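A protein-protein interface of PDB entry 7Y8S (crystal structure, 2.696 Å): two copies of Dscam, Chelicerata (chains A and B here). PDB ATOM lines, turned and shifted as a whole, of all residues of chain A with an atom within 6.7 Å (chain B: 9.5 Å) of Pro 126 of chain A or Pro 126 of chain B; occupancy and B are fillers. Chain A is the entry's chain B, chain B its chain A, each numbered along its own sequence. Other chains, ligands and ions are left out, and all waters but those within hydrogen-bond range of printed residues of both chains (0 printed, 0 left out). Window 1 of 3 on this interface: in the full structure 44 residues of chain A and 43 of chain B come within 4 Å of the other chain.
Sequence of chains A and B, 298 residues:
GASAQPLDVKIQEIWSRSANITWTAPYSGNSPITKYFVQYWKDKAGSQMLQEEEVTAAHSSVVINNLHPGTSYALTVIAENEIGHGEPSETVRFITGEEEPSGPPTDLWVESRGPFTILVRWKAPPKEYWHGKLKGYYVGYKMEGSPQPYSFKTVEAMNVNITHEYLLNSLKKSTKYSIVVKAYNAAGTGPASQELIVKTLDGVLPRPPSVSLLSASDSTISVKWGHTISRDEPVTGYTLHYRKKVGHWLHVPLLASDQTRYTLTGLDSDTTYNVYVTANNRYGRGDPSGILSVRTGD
The backbone carbonyl oxygen (O) of Pro 104 of chain A is in hydrogen-bond range of the side-chain hydroxyl (OH) of Tyr 129 of chain B.
The backbone carbonyl oxygen of Pro 104 of chain B lies within hydrogen-bond range of the side-chain hydroxyl of Tyr 129 of chain A, at 2.9 Å.
The indole nitrogen of Trp 130 of chain A is in hydrogen-bond range of the backbone carbonyl oxygen of Pro 125 of chain A.
The backbone NH (N) of Ser 102 of chain B sits at hydrogen-bond distance from the backbone carbonyl oxygen (O) of Tyr 129 of chain B (3.1 Å).
The indole nitrogen (NE1) of Trp 130 of chain B lies within hydrogen-bond range of the backbone carbonyl oxygen (O) of Pro 125 of chain B (2.7 Å).
O of Pro 126 of chain A sits close to NE1 of Trp 130 of chain A, at 3.5 Å.
CA of Gly 103 of chain A touches OH of Tyr 129 of chain B (3.3 Å).
CB of Glu 128 of chain B touches CG2 of Thr 106 of chain A, at 3.8 Å.
Tyr 129 of chain B touches Thr 106 of chain A.
CB of Pro 125 of chain A touches OH of Tyr 129 of chain B, 3.8 Å away.
Pro 126 of chain A touches Pro 126 of chain B.
CD of Pro 126 of chain A touches OH of Tyr 129 of chain B, at 3.6 Å.
Tyr 129 of chain A touches Gly 103 of chain B.
OH of Tyr 129 of chain A touches CB of Pro 125 of chain B, at 3.9 Å.
Tyr 129 of chain A touches Pro 126 of chain B.
Tyr 129 of chain B touches Tyr 129 of chain A.
Of chain B, only Pro 126 and Tyr 129 come within 4 Å of Pro 126 of chain A.
Pro 126 of chain B touches just these residues of chain A: Pro 126 (3.4 Å) and Tyr 129 (3.6 Å).
Pro 125 of chain A touches just one residue of chain B: Tyr 129 (3.8 Å).
Of chain B, only Gly 103, Pro 104, Pro 125, Pro 126 and Tyr 129 come within 4 Å of Tyr 129 of chain A.
Of the printed residues of chain A, Pro 125 of chain B touches Tyr 129 (3.9 Å).
Of the printed residues of chain A, Glu 128 of chain B touches Thr 106 (3.8 Å).
Of the printed residues of chain A, Pro 104 of chain B touches Tyr 129 (2.9 Å).
Printed residues of chain B within 4 Å of Pro 104 of chain A: Tyr 129 (2.9 Å).
Trp 130 of chain A touches none of the printed residues of chain B.
The nearest residue of chain B that does not touch Pro 126 of chain A is Glu 128 of chain B (5.7 Å).
The nearest printed residue of chain A that does not touch Tyr 129 of chain B is Ala 124 of chain A (6.2 Å).
Hydrophobic or aromatic side chains of chain B that line the printed part of chain A: Pro 104, Pro 125, Pro 126 and Tyr 129.
Among the printed residues, no Asp or Glu carboxylate lies within 4 Å of a Lys or Arg side-chain nitrogen of the other chain.
Pro 104 of chain A touches Tyr 129 of chain B, and with the chains exchanged Tyr 129 of chain A touches Pro 104 of chain B.
Thr 106 of chain A touches Glu 128 of chain B, but with the chains exchanged Glu 128 of chain A does not touch Thr 106 of chain B (4.1 Å).
Thr 106 of chain A touches Tyr 129 of chain B, but with the chains exchanged Tyr 129 of chain A does not touch Thr 106 of chain B (4.2 Å).
Pro 125 of chain A touches Tyr 129 of chain B, and with the chains exchanged Tyr 129 of chain A touches Pro 125 of chain B.
Of the 12 pairs that touch across the chains among the printed residues, 10 have their exchanged pair printed and touching as well.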
ATOM      1  N   GLY A 103     -15.332 -11.452  23.278  1.00  0.00           N
ATOM      2  CA  GLY A 103     -15.587 -10.433  22.286  1.00  0.00           C
ATOM      3  C   GLY A 103     -17.027  -9.954  22.313  1.00  0.00           C
ATOM      4  O   GLY A 103     -17.958 -10.717  22.585  1.00  0.00           O
ATOM      5  N   PRO A 104     -17.238  -8.674  22.034  1.00  0.00           N
ATOM      6  CA  PRO A 104     -18.596  -8.127  22.049  1.00  0.00           C
ATOM      7  C   PRO A 104     -19.315  -8.418  20.745  1.00  0.00           C
ATOM      8  O   PRO A 104     -18.677  -8.756  19.736  1.00  0.00           O
ATOM      9  CB  PRO A 104     -18.354  -6.623  22.215  1.00  0.00           C
ATOM     10  CG  PRO A 104     -17.068  -6.405  21.467  1.00  0.00           C
ATOM     11  CD  PRO A 104     -16.231  -7.640  21.733  1.00  0.00           C
ATOM     12  N   THR A 106     -21.118  -7.262  17.262  1.00  0.00           N
ATOM     13  CA  THR A 106     -20.662  -6.249  16.322  1.00  0.00           C
ATOM     14  C   THR A 106     -21.795  -5.815  15.404  1.00  0.00           C
ATOM     15  O   THR A 106     -22.895  -6.377  15.414  1.00  0.00           O
ATOM     16  CB  THR A 106     -19.481  -6.751  15.486  1.00  0.00           C
ATOM     17  OG1 THR A 106     -19.792  -8.046  14.950  1.00  0.00           O
ATOM     18  CG2 THR A 106     -18.231  -6.830  16.347  1.00  0.00           C
ATOM     19  N   ALA A 124     -23.660 -11.701  15.899  1.00  0.00           N
ATOM     20  CA  ALA A 124     -23.017 -12.355  17.022  1.00  0.00           C
ATOM     21  C   ALA A 124     -21.507 -12.152  16.956  1.00  0.00           C
ATOM     22  O   ALA A 124     -20.940 -11.990  15.874  1.00  0.00           O
ATOM     23  CB  ALA A 124     -23.327 -13.847  17.022  1.00  0.00           C
ATOM     24  N   PRO A 125     -20.830 -12.163  18.099  1.00  0.00           N
ATOM     25  CA  PRO A 125     -19.377 -12.258  18.079  1.00  0.00           C
ATOM     26  C   PRO A 125     -18.966 -13.548  17.400  1.00  0.00           C
ATOM     27  O   PRO A 125     -19.751 -14.509  17.354  1.00  0.00           O
ATOM     28  CB  PRO A 125     -18.993 -12.254  19.567  1.00  0.00           C
ATOM     29  CG  PRO A 125     -20.222 -12.676  20.282  1.00  0.00           C
ATOM     30  CD  PRO A 125     -21.366 -12.150  19.471  1.00  0.00           C
ATOM     31  N   PRO A 126     -17.761 -13.608  16.842  1.00  0.00           N
ATOM     32  CA  PRO A 126     -17.352 -14.810  16.106  1.00  0.00           C
ATOM     33  C   PRO A 126     -17.293 -16.022  17.021  1.00  0.00           C
ATOM     34  O   PRO A 126     -16.946 -15.917  18.201  1.00  0.00           O
ATOM     35  CB  PRO A 126     -15.973 -14.436  15.557  1.00  0.00           C
ATOM     36  CG  PRO A 126     -15.965 -12.930  15.573  1.00  0.00           C
ATOM     37  CD  PRO A 126     -16.743 -12.548  16.781  1.00  0.00           C
ATOM     38  N   LYS A 127     -17.661 -17.182  16.463  1.00  0.00           N
ATOM     39  CA  LYS A 127     -17.768 -18.405  17.256  1.00  0.00           C
ATOM     40  C   LYS A 127     -16.498 -18.673  18.051  1.00  0.00           C
ATOM     41  O   LYS A 127     -16.556 -19.154  19.190  1.00  0.00           O
ATOM     42  CB  LYS A 127     -18.088 -19.595  16.346  1.00  0.00           C
ATOM     43  CG  LYS A 127     -19.534 -19.646  15.865  1.00  0.00           C
ATOM     44  CD  LYS A 127     -20.266 -20.890  16.373  1.00  0.00           C
ATOM     45  CE  LYS A 127     -21.528 -21.173  15.557  1.00  0.00           C
ATOM     46  NZ  LYS A 127     -21.253 -21.940  14.308  1.00  0.00           N
ATOM     47  N   GLU A 128     -15.341 -18.341  17.475  1.00  0.00           N
ATOM     48  CA  GLU A 128     -14.063 -18.600  18.125  1.00  0.00           C
ATOM     49  C   GLU A 128     -13.902 -17.843  19.440  1.00  0.00           C
ATOM     50  O   GLU A 128     -13.062 -18.229  20.261  1.00  0.00           O
ATOM     51  CB  GLU A 128     -12.919 -18.246  17.175  1.00  0.00           C
ATOM     52  CG  GLU A 128     -13.010 -18.903  15.794  1.00  0.00           C
ATOM     53  CD  GLU A 128     -14.017 -18.230  14.873  1.00  0.00           C
ATOM     54  OE1 GLU A 128     -14.674 -17.264  15.315  1.00  0.00           O
ATOM     55  OE2 GLU A 128     -14.156 -18.666  13.711  1.00  0.00           O
ATOM     56  N   TYR A 129     -14.684 -16.786  19.665  1.00  0.00           N
ATOM     57  CA  TYR A 129     -14.595 -16.002  20.893  1.00  0.00           C
ATOM     58  C   TYR A 129     -15.672 -16.354  21.908  1.00  0.00           C
ATOM     59  O   TYR A 129     -15.760 -15.691  22.946  1.00  0.00           O
ATOM     60  CB  TYR A 129     -14.669 -14.505  20.582  1.00  0.00           C
ATOM     61  CG  TYR A 129     -13.509 -13.970  19.772  1.00  0.00           C
ATOM     62  CD1 TYR A 129     -12.315 -14.669  19.682  1.00  0.00           C
ATOM     63  CD2 TYR A 129     -13.614 -12.764  19.095  1.00  0.00           C
ATOM     64  CE1 TYR A 129     -11.258 -14.181  18.943  1.00  0.00           C
ATOM     65  CE2 TYR A 129     -12.562 -12.270  18.352  1.00  0.00           C
ATOM     66  CZ  TYR A 129     -11.387 -12.982  18.282  1.00  0.00           C
ATOM     67  OH  TYR A 129     -10.336 -12.494  17.543  1.00  0.00           O
ATOM     68  N   TRP A 130     -16.492 -17.373  21.636  1.00  0.00           N
ATOM     69  CA  TRP A 130     -17.568 -17.729  22.557  1.00  0.00           C
ATOM     70  C   TRP A 130     -17.027 -18.426  23.800  1.00  0.00           C
ATOM     71  O   TRP A 130     -17.461 -18.137  24.923  1.00  0.00           O
ATOM     72  CB  TRP A 130     -18.586 -18.630  21.861  1.00  0.00           C
ATOM     73  CG  TRP A 130     -19.401 -17.984  20.794  1.00  0.00           C
ATOM     74  CD1 TRP A 130     -19.237 -16.738  20.260  1.00  0.00           C
ATOM     75  CD2 TRP A 130     -20.525 -18.561  20.126  1.00  0.00           C
ATOM     76  NE1 TRP A 130     -20.192 -16.507  19.297  1.00  0.00           N
ATOM     77  CE2 TRP A 130     -20.994 -17.613  19.198  1.00  0.00           C
ATOM     78  CE3 TRP A 130     -21.181 -19.790  20.225  1.00  0.00           C
ATOM     79  CZ2 TRP A 130     -22.089 -17.860  18.374  1.00  0.00           C
ATOM     80  CZ3 TRP A 130     -22.261 -20.032  19.408  1.00  0.00           C
ATOM     81  CH2 TRP A 130     -22.707 -19.073  18.495  1.00  0.00           C
ATOM     82  N   HIS A 131     -16.103 -19.373  23.615  1.00  0.00           N
ATOM     83  CA  HIS A 131     -15.552 -20.176  24.710  1.00  0.00           C
ATOM     84  C   HIS A 131     -16.652 -20.915  25.463  1.00  0.00           C
ATOM     85  O   HIS A 131     -16.535 -21.175  26.664  1.00  0.00           O
ATOM     86  CB  HIS A 131     -14.722 -19.319  25.670  1.00  0.00           C
ATOM     87  CG  HIS A 131     -13.737 -18.428  24.979  1.00  0.00           C
ATOM     88  ND1 HIS A 131     -13.214 -18.719  23.737  1.00  0.00           N
ATOM     89  CD2 HIS A 131     -13.192 -17.245  25.348  1.00  0.00           C
ATOM     90  CE1 HIS A 131     -12.383 -17.760  23.375  1.00  0.00           C
ATOM     91  NE2 HIS A 131     -12.352 -16.852  24.335  1.00  0.00           N
ATOM     92  N   PRO B 101      -5.794  -3.780  18.000  1.00  0.00           N
ATOM     93  CA  PRO B 101      -6.737  -4.884  17.777  1.00  0.00           C
ATOM     94  C   PRO B 101      -7.159  -5.500  19.100  1.00  0.00           C
ATOM     95  O   PRO B 101      -6.375  -5.581  20.049  1.00  0.00           O
ATOM     96  CB  PRO B 101      -5.934  -5.868  16.918  1.00  0.00           C
ATOM     97  CG  PRO B 101      -4.901  -5.018  16.234  1.00  0.00           C
ATOM     98  CD  PRO B 101      -4.548  -3.950  17.235  1.00  0.00           C
ATOM     99  N   SER B 102      -8.421  -5.914  19.166  1.00  0.00           N
ATOM    100  CA  SER B 102      -9.015  -6.395  20.405  1.00  0.00           C
ATOM    101  C   SER B 102      -9.266  -7.896  20.401  1.00  0.00           C
ATOM    102  O   SER B 102      -9.797  -8.427  21.384  1.00  0.00           O
ATOM    103  CB  SER B 102     -10.322  -5.640  20.685  1.00  0.00           C
ATOM    104  OG  SER B 102     -11.137  -5.586  19.526  1.00  0.00           O
ATOM    105  N   GLY B 103      -8.901  -8.594  19.330  1.00  0.00           N
ATOM    106  CA  GLY B 103      -9.018 -10.033  19.286  1.00  0.00           C
ATOM    107  C   GLY B 103      -7.731 -10.675  18.809  1.00  0.00           C
ATOM    108  O   GLY B 103      -6.950 -10.064  18.076  1.00  0.00           O
ATOM    109  N   PRO B 104      -7.478 -11.913  19.227  1.00  0.00           N
ATOM    110  CA  PRO B 104      -6.270 -12.625  18.779  1.00  0.00           C
ATOM    111  C   PRO B 104      -6.497 -13.282  17.433  1.00  0.00           C
ATOM    112  O   PRO B 104      -7.642 -13.368  16.967  1.00  0.00           O
ATOM    113  CB  PRO B 104      -6.063 -13.676  19.875  1.00  0.00           C
ATOM    114  CG  PRO B 104      -7.449 -13.974  20.346  1.00  0.00           C
ATOM    115  CD  PRO B 104      -8.241 -12.689  20.221  1.00  0.00           C
ATOM    116  N   PRO B 105      -5.436 -13.754  16.774  1.00  0.00           N
ATOM    117  CA  PRO B 105      -5.624 -14.594  15.583  1.00  0.00           C
ATOM    118  C   PRO B 105      -6.316 -15.898  15.947  1.00  0.00           C
ATOM    119  O   PRO B 105      -6.234 -16.377  17.081  1.00  0.00           O
ATOM    120  CB  PRO B 105      -4.196 -14.840  15.083  1.00  0.00           C
ATOM    121  CG  PRO B 105      -3.367 -13.780  15.719  1.00  0.00           C
ATOM    122  CD  PRO B 105      -4.017 -13.461  17.028  1.00  0.00           C
ATOM    123  N   THR B 106      -7.009 -16.470  14.970  1.00  0.00           N
ATOM    124  CA  THR B 106      -7.806 -17.670  15.174  1.00  0.00           C
ATOM    125  C   THR B 106      -7.263 -18.820  14.336  1.00  0.00           C
ATOM    126  O   THR B 106      -6.424 -18.641  13.448  1.00  0.00           O
ATOM    127  CB  THR B 106      -9.282 -17.426  14.826  1.00  0.00           C
ATOM    128  OG1 THR B 106      -9.435 -17.348  13.402  1.00  0.00           O
ATOM    129  CG2 THR B 106      -9.773 -16.132  15.456  1.00  0.00           C
ATOM    130  N   ASP B 107      -7.774 -20.015  14.639  1.00  0.00           N
ATOM    131  CA  ASP B 107      -7.453 -21.236  13.903  1.00  0.00           C
ATOM    132  C   ASP B 107      -5.943 -21.454  13.845  1.00  0.00           C
ATOM    133  O   ASP B 107      -5.344 -21.602  12.775  1.00  0.00           O
ATOM    134  CB  ASP B 107      -8.087 -21.216  12.510  1.00  0.00           C
ATOM    135  CG  ASP B 107      -9.605 -21.336  12.571  1.00  0.00           C
ATOM    136  OD1 ASP B 107     -10.282 -21.067  11.561  1.00  0.00           O
ATOM    137  OD2 ASP B 107     -10.125 -21.698  13.648  1.00  0.00           O
ATOM    138  N   LYS B 123      -5.433 -17.854  10.880  1.00  0.00           N
ATOM    139  CA  LYS B 123      -6.303 -16.932  10.174  1.00  0.00           C
ATOM    140  C   LYS B 123      -6.348 -15.599  10.908  1.00  0.00           C
ATOM    141  O   LYS B 123      -6.162 -15.530  12.129  1.00  0.00           O
ATOM    142  CB  LYS B 123      -7.710 -17.506  10.016  1.00  0.00           C
ATOM    143  CG  LYS B 123      -7.826 -18.378   8.772  1.00  0.00           C
ATOM    144  CD  LYS B 123      -8.706 -19.580   9.018  1.00  0.00           C
ATOM    145  CE  LYS B 123     -10.108 -19.324   8.504  1.00  0.00           C
ATOM    146  NZ  LYS B 123     -11.140 -20.165   9.179  1.00  0.00           N
ATOM    147  N   ALA B 124      -6.573 -14.535  10.144  1.00  0.00           N
ATOM    148  CA  ALA B 124      -6.598 -13.205  10.723  1.00  0.00           C
ATOM    149  C   ALA B 124      -7.778 -13.078  11.681  1.00  0.00           C
ATOM    150  O   ALA B 124      -8.782 -13.780  11.536  1.00  0.00           O
ATOM    151  CB  ALA B 124      -6.703 -12.146   9.633  1.00  0.00           C
ATOM    152  N   PRO B 125      -7.678 -12.210  12.680  1.00  0.00           N
ATOM    153  CA  PRO B 125      -8.845 -11.912  13.502  1.00  0.00           C
ATOM    154  C   PRO B 125      -9.902 -11.216  12.663  1.00  0.00           C
ATOM    155  O   PRO B 125      -9.571 -10.555  11.666  1.00  0.00           O
ATOM    156  CB  PRO B 125      -8.290 -10.991  14.604  1.00  0.00           C
ATOM    157  CG  PRO B 125      -7.016 -10.452  14.062  1.00  0.00           C
ATOM    158  CD  PRO B 125      -6.471 -11.500  13.138  1.00  0.00           C
ATOM    159  N   PRO B 126     -11.179 -11.347  13.021  1.00  0.00           N
ATOM    160  CA  PRO B 126     -12.234 -10.715  12.219  1.00  0.00           C
ATOM    161  C   PRO B 126     -12.038  -9.206  12.153  1.00  0.00           C
ATOM    162  O   PRO B 126     -11.743  -8.555  13.159  1.00  0.00           O
ATOM    163  CB  PRO B 126     -13.518 -11.085  12.970  1.00  0.00           C
ATOM    164  CG  PRO B 126     -13.119 -12.225  13.881  1.00  0.00           C
ATOM    165  CD  PRO B 126     -11.712 -11.953  14.250  1.00  0.00           C
ATOM    166  N   LYS B 127     -12.207  -8.658  10.941  1.00  0.00           N
ATOM    167  CA  LYS B 127     -11.876  -7.254  10.675  1.00  0.00           C
ATOM    168  C   LYS B 127     -12.616  -6.302  11.598  1.00  0.00           C
ATOM    169  O   LYS B 127     -12.109  -5.213  11.908  1.00  0.00           O
ATOM    170  CB  LYS B 127     -12.162  -6.896   9.206  1.00  0.00           C
ATOM    171  CG  LYS B 127     -11.379  -5.660   8.692  1.00  0.00           C
ATOM    172  CD  LYS B 127     -12.048  -4.305   8.990  1.00  0.00           C
ATOM    173  CE  LYS B 127     -11.101  -3.125   8.749  1.00  0.00           C
ATOM    174  NZ  LYS B 127     -10.407  -2.740  10.023  1.00  0.00           N
ATOM    175  N   GLU B 128     -13.797  -6.706  12.066  1.00  0.00           N
ATOM    176  CA  GLU B 128     -14.513  -5.896  13.040  1.00  0.00           C
ATOM    177  C   GLU B 128     -13.687  -5.643  14.298  1.00  0.00           C
ATOM    178  O   GLU B 128     -14.005  -4.725  15.064  1.00  0.00           O
ATOM    179  CB  GLU B 128     -15.835  -6.567  13.418  1.00  0.00           C
ATOM    180  CG  GLU B 128     -16.841  -6.728  12.272  1.00  0.00           C
ATOM    181  CD  GLU B 128     -16.582  -7.955  11.413  1.00  0.00           C
ATOM    182  OE1 GLU B 128     -15.676  -8.743  11.761  1.00  0.00           O
ATOM    183  OE2 GLU B 128     -17.288  -8.134  10.395  1.00  0.00           O
ATOM    184  N   TYR B 129     -12.640  -6.437  14.527  1.00  0.00           N
ATOM    185  CA  TYR B 129     -11.802  -6.315  15.711  1.00  0.00           C
ATOM    186  C   TYR B 129     -10.441  -5.693  15.426  1.00  0.00           C
ATOM    187  O   TYR B 129      -9.621  -5.599  16.346  1.00  0.00           O
ATOM    188  CB  TYR B 129     -11.601  -7.688  16.363  1.00  0.00           C
ATOM    189  CG  TYR B 129     -12.810  -8.246  17.083  1.00  0.00           C
ATOM    190  CD1 TYR B 129     -13.958  -8.595  16.393  1.00  0.00           C
ATOM    191  CD2 TYR B 129     -12.789  -8.445  18.454  1.00  0.00           C
ATOM    192  CE1 TYR B 129     -15.059  -9.115  17.050  1.00  0.00           C
ATOM    193  CE2 TYR B 129     -13.887  -8.963  19.120  1.00  0.00           C
ATOM    194  CZ  TYR B 129     -15.016  -9.295  18.412  1.00  0.00           C
ATOM    195  OH  TYR B 129     -16.104  -9.811  19.076  1.00  0.00           O
ATOM    196  N   TRP B 130     -10.167  -5.279  14.185  1.00  0.00           N
ATOM    197  CA  TRP B 130      -8.872  -4.676  13.876  1.00  0.00           C
ATOM    198  C   TRP B 130      -8.740  -3.294  14.505  1.00  0.00           C
ATOM    199  O   TRP B 130      -7.701  -2.966  15.093  1.00  0.00           O
ATOM    200  CB  TRP B 130      -8.669  -4.583  12.363  1.00  0.00           C
ATOM    201  CG  TRP B 130      -8.527  -5.901  11.656  1.00  0.00           C
ATOM    202  CD1 TRP B 130      -8.739  -7.147  12.178  1.00  0.00           C
ATOM    203  CD2 TRP B 130      -8.146  -6.099  10.289  1.00  0.00           C
ATOM    204  NE1 TRP B 130      -8.516  -8.105  11.216  1.00  0.00           N
ATOM    205  CE2 TRP B 130      -8.150  -7.485  10.049  1.00  0.00           C
ATOM    206  CE3 TRP B 130      -7.802  -5.236   9.245  1.00  0.00           C
ATOM    207  CZ2 TRP B 130      -7.825  -8.028   8.809  1.00  0.00           C
ATOM    208  CZ3 TRP B 130      -7.477  -5.777   8.017  1.00  0.00           C
ATOM    209  CH2 TRP B 130      -7.490  -7.159   7.809  1.00  0.00           C
ATOM    210  N   HIS B 131      -9.780  -2.463  14.371  1.00  0.00           N
ATOM    211  CA  HIS B 131      -9.748  -1.069  14.816  1.00  0.00           C
ATOM    212  C   HIS B 131      -8.633  -0.296  14.122  1.00  0.00           C
ATOM    213  O   HIS B 131      -8.060   0.641  14.685  1.00  0.00           O
ATOM    214  CB  HIS B 131      -9.617  -0.988  16.336  1.00  0.00           C
ATOM    215  CG  HIS B 131     -10.629  -1.818  17.062  1.00  0.00           C
ATOM    216  ND1 HIS B 131     -11.864  -2.113  16.527  1.00  0.00           N
ATOM    217  CD2 HIS B 131     -10.584  -2.432  18.267  1.00  0.00           C
ATOM    218  CE1 HIS B 131     -12.543  -2.860  17.380  1.00  0.00           C
ATOM    219  NE2 HIS B 131     -11.787  -3.069  18.443  1.00  0.00           N
ATOM    220  N   GLY B 132      -8.331  -0.691  12.887  1.00  0.00           N
ATOM    221  CA  GLY B 132      -7.238  -0.125  12.125  1.00  0.00           C
ATOM    222  C   GLY B 132      -6.543  -1.177  11.286  1.00  0.00           C
ATOM    223  O   GLY B 132      -6.343  -2.305  11.750  1.00  0.00           O
ATOM    224  N   LEU B 134      -4.325  -3.764   9.661  1.00  0.00           N
ATOM    225  CA  LEU B 134      -3.232  -4.499  10.282  1.00  0.00           C
ATOM    226  C   LEU B 134      -1.925  -4.242   9.547  1.00  0.00           C
ATOM    227  O   LEU B 134      -1.878  -4.262   8.313  1.00  0.00           O
ATOM    228  CB  LEU B 134      -3.537  -5.995  10.297  1.00  0.00           C
ATOM    229  CG  LEU B 134      -4.731  -6.458  11.132  1.00  0.00           C
ATOM    230  CD1 LEU B 134      -4.771  -7.982  11.177  1.00  0.00           C
ATOM    231  CD2 LEU B 134      -4.678  -5.869  12.537  1.00  0.00           C
ATOM    232  N   TYR B 137       1.975  -9.285  11.942  1.00  0.00           N
ATOM    233  CA  TYR B 137       1.787 -10.140  13.105  1.00  0.00           C
ATOM    234  C   TYR B 137       3.121 -10.368  13.801  1.00  0.00           C
ATOM    235  O   TYR B 137       4.189 -10.295  13.188  1.00  0.00           O
ATOM    236  CB  TYR B 137       1.181 -11.502  12.735  1.00  0.00           C
ATOM    237  CG  TYR B 137      -0.151 -11.431  12.046  1.00  0.00           C
ATOM    238  CD1 TYR B 137      -1.334 -11.486  12.771  1.00  0.00           C
ATOM    239  CD2 TYR B 137      -0.229 -11.310  10.665  1.00  0.00           C
ATOM    240  CE1 TYR B 137      -2.560 -11.420  12.140  1.00  0.00           C
ATOM    241  CE2 TYR B 137      -1.445 -11.243  10.024  1.00  0.00           C
ATOM    242  CZ  TYR B 137      -2.608 -11.299  10.764  1.00  0.00           C
ATOM    243  OH  TYR B 137      -3.822 -11.232  10.125  1.00  0.00           O
ATOM    244  N   HIS B 164      -2.425 -17.294   6.876  1.00  0.00           N
ATOM    245  CA  HIS B 164      -1.112 -16.724   7.127  1.00  0.00           C
ATOM    246  C   HIS B 164      -0.213 -17.784   7.741  1.00  0.00           C
ATOM    247  O   HIS B 164      -0.681 -18.666   8.465  1.00  0.00           O
ATOM    248  CB  HIS B 164      -1.199 -15.517   8.060  1.00  0.00           C
ATOM    249  CG  HIS B 164      -2.164 -14.470   7.601  1.00  0.00           C
ATOM    250  ND1 HIS B 164      -3.524 -14.575   7.794  1.00  0.00           N
ATOM    251  CD2 HIS B 164      -1.964 -13.299   6.953  1.00  0.00           C
ATOM    252  CE1 HIS B 164      -4.122 -13.510   7.288  1.00  0.00           C
ATOM    253  NE2 HIS B 164      -3.196 -12.720   6.772  1.00  0.00           N
ATOM    254  N   ALA B 183      -1.692 -10.003  16.456  1.00  0.00           N
ATOM    255  CA  ALA B 183      -1.837  -9.034  15.380  1.00  0.00           C
ATOM    256  C   ALA B 183      -1.453  -7.649  15.884  1.00  0.00           C
ATOM    257  O   ALA B 183      -1.524  -7.363  17.084  1.00  0.00           O
ATOM    258  CB  ALA B 183      -3.270  -9.023  14.846  1.00  0.00           C
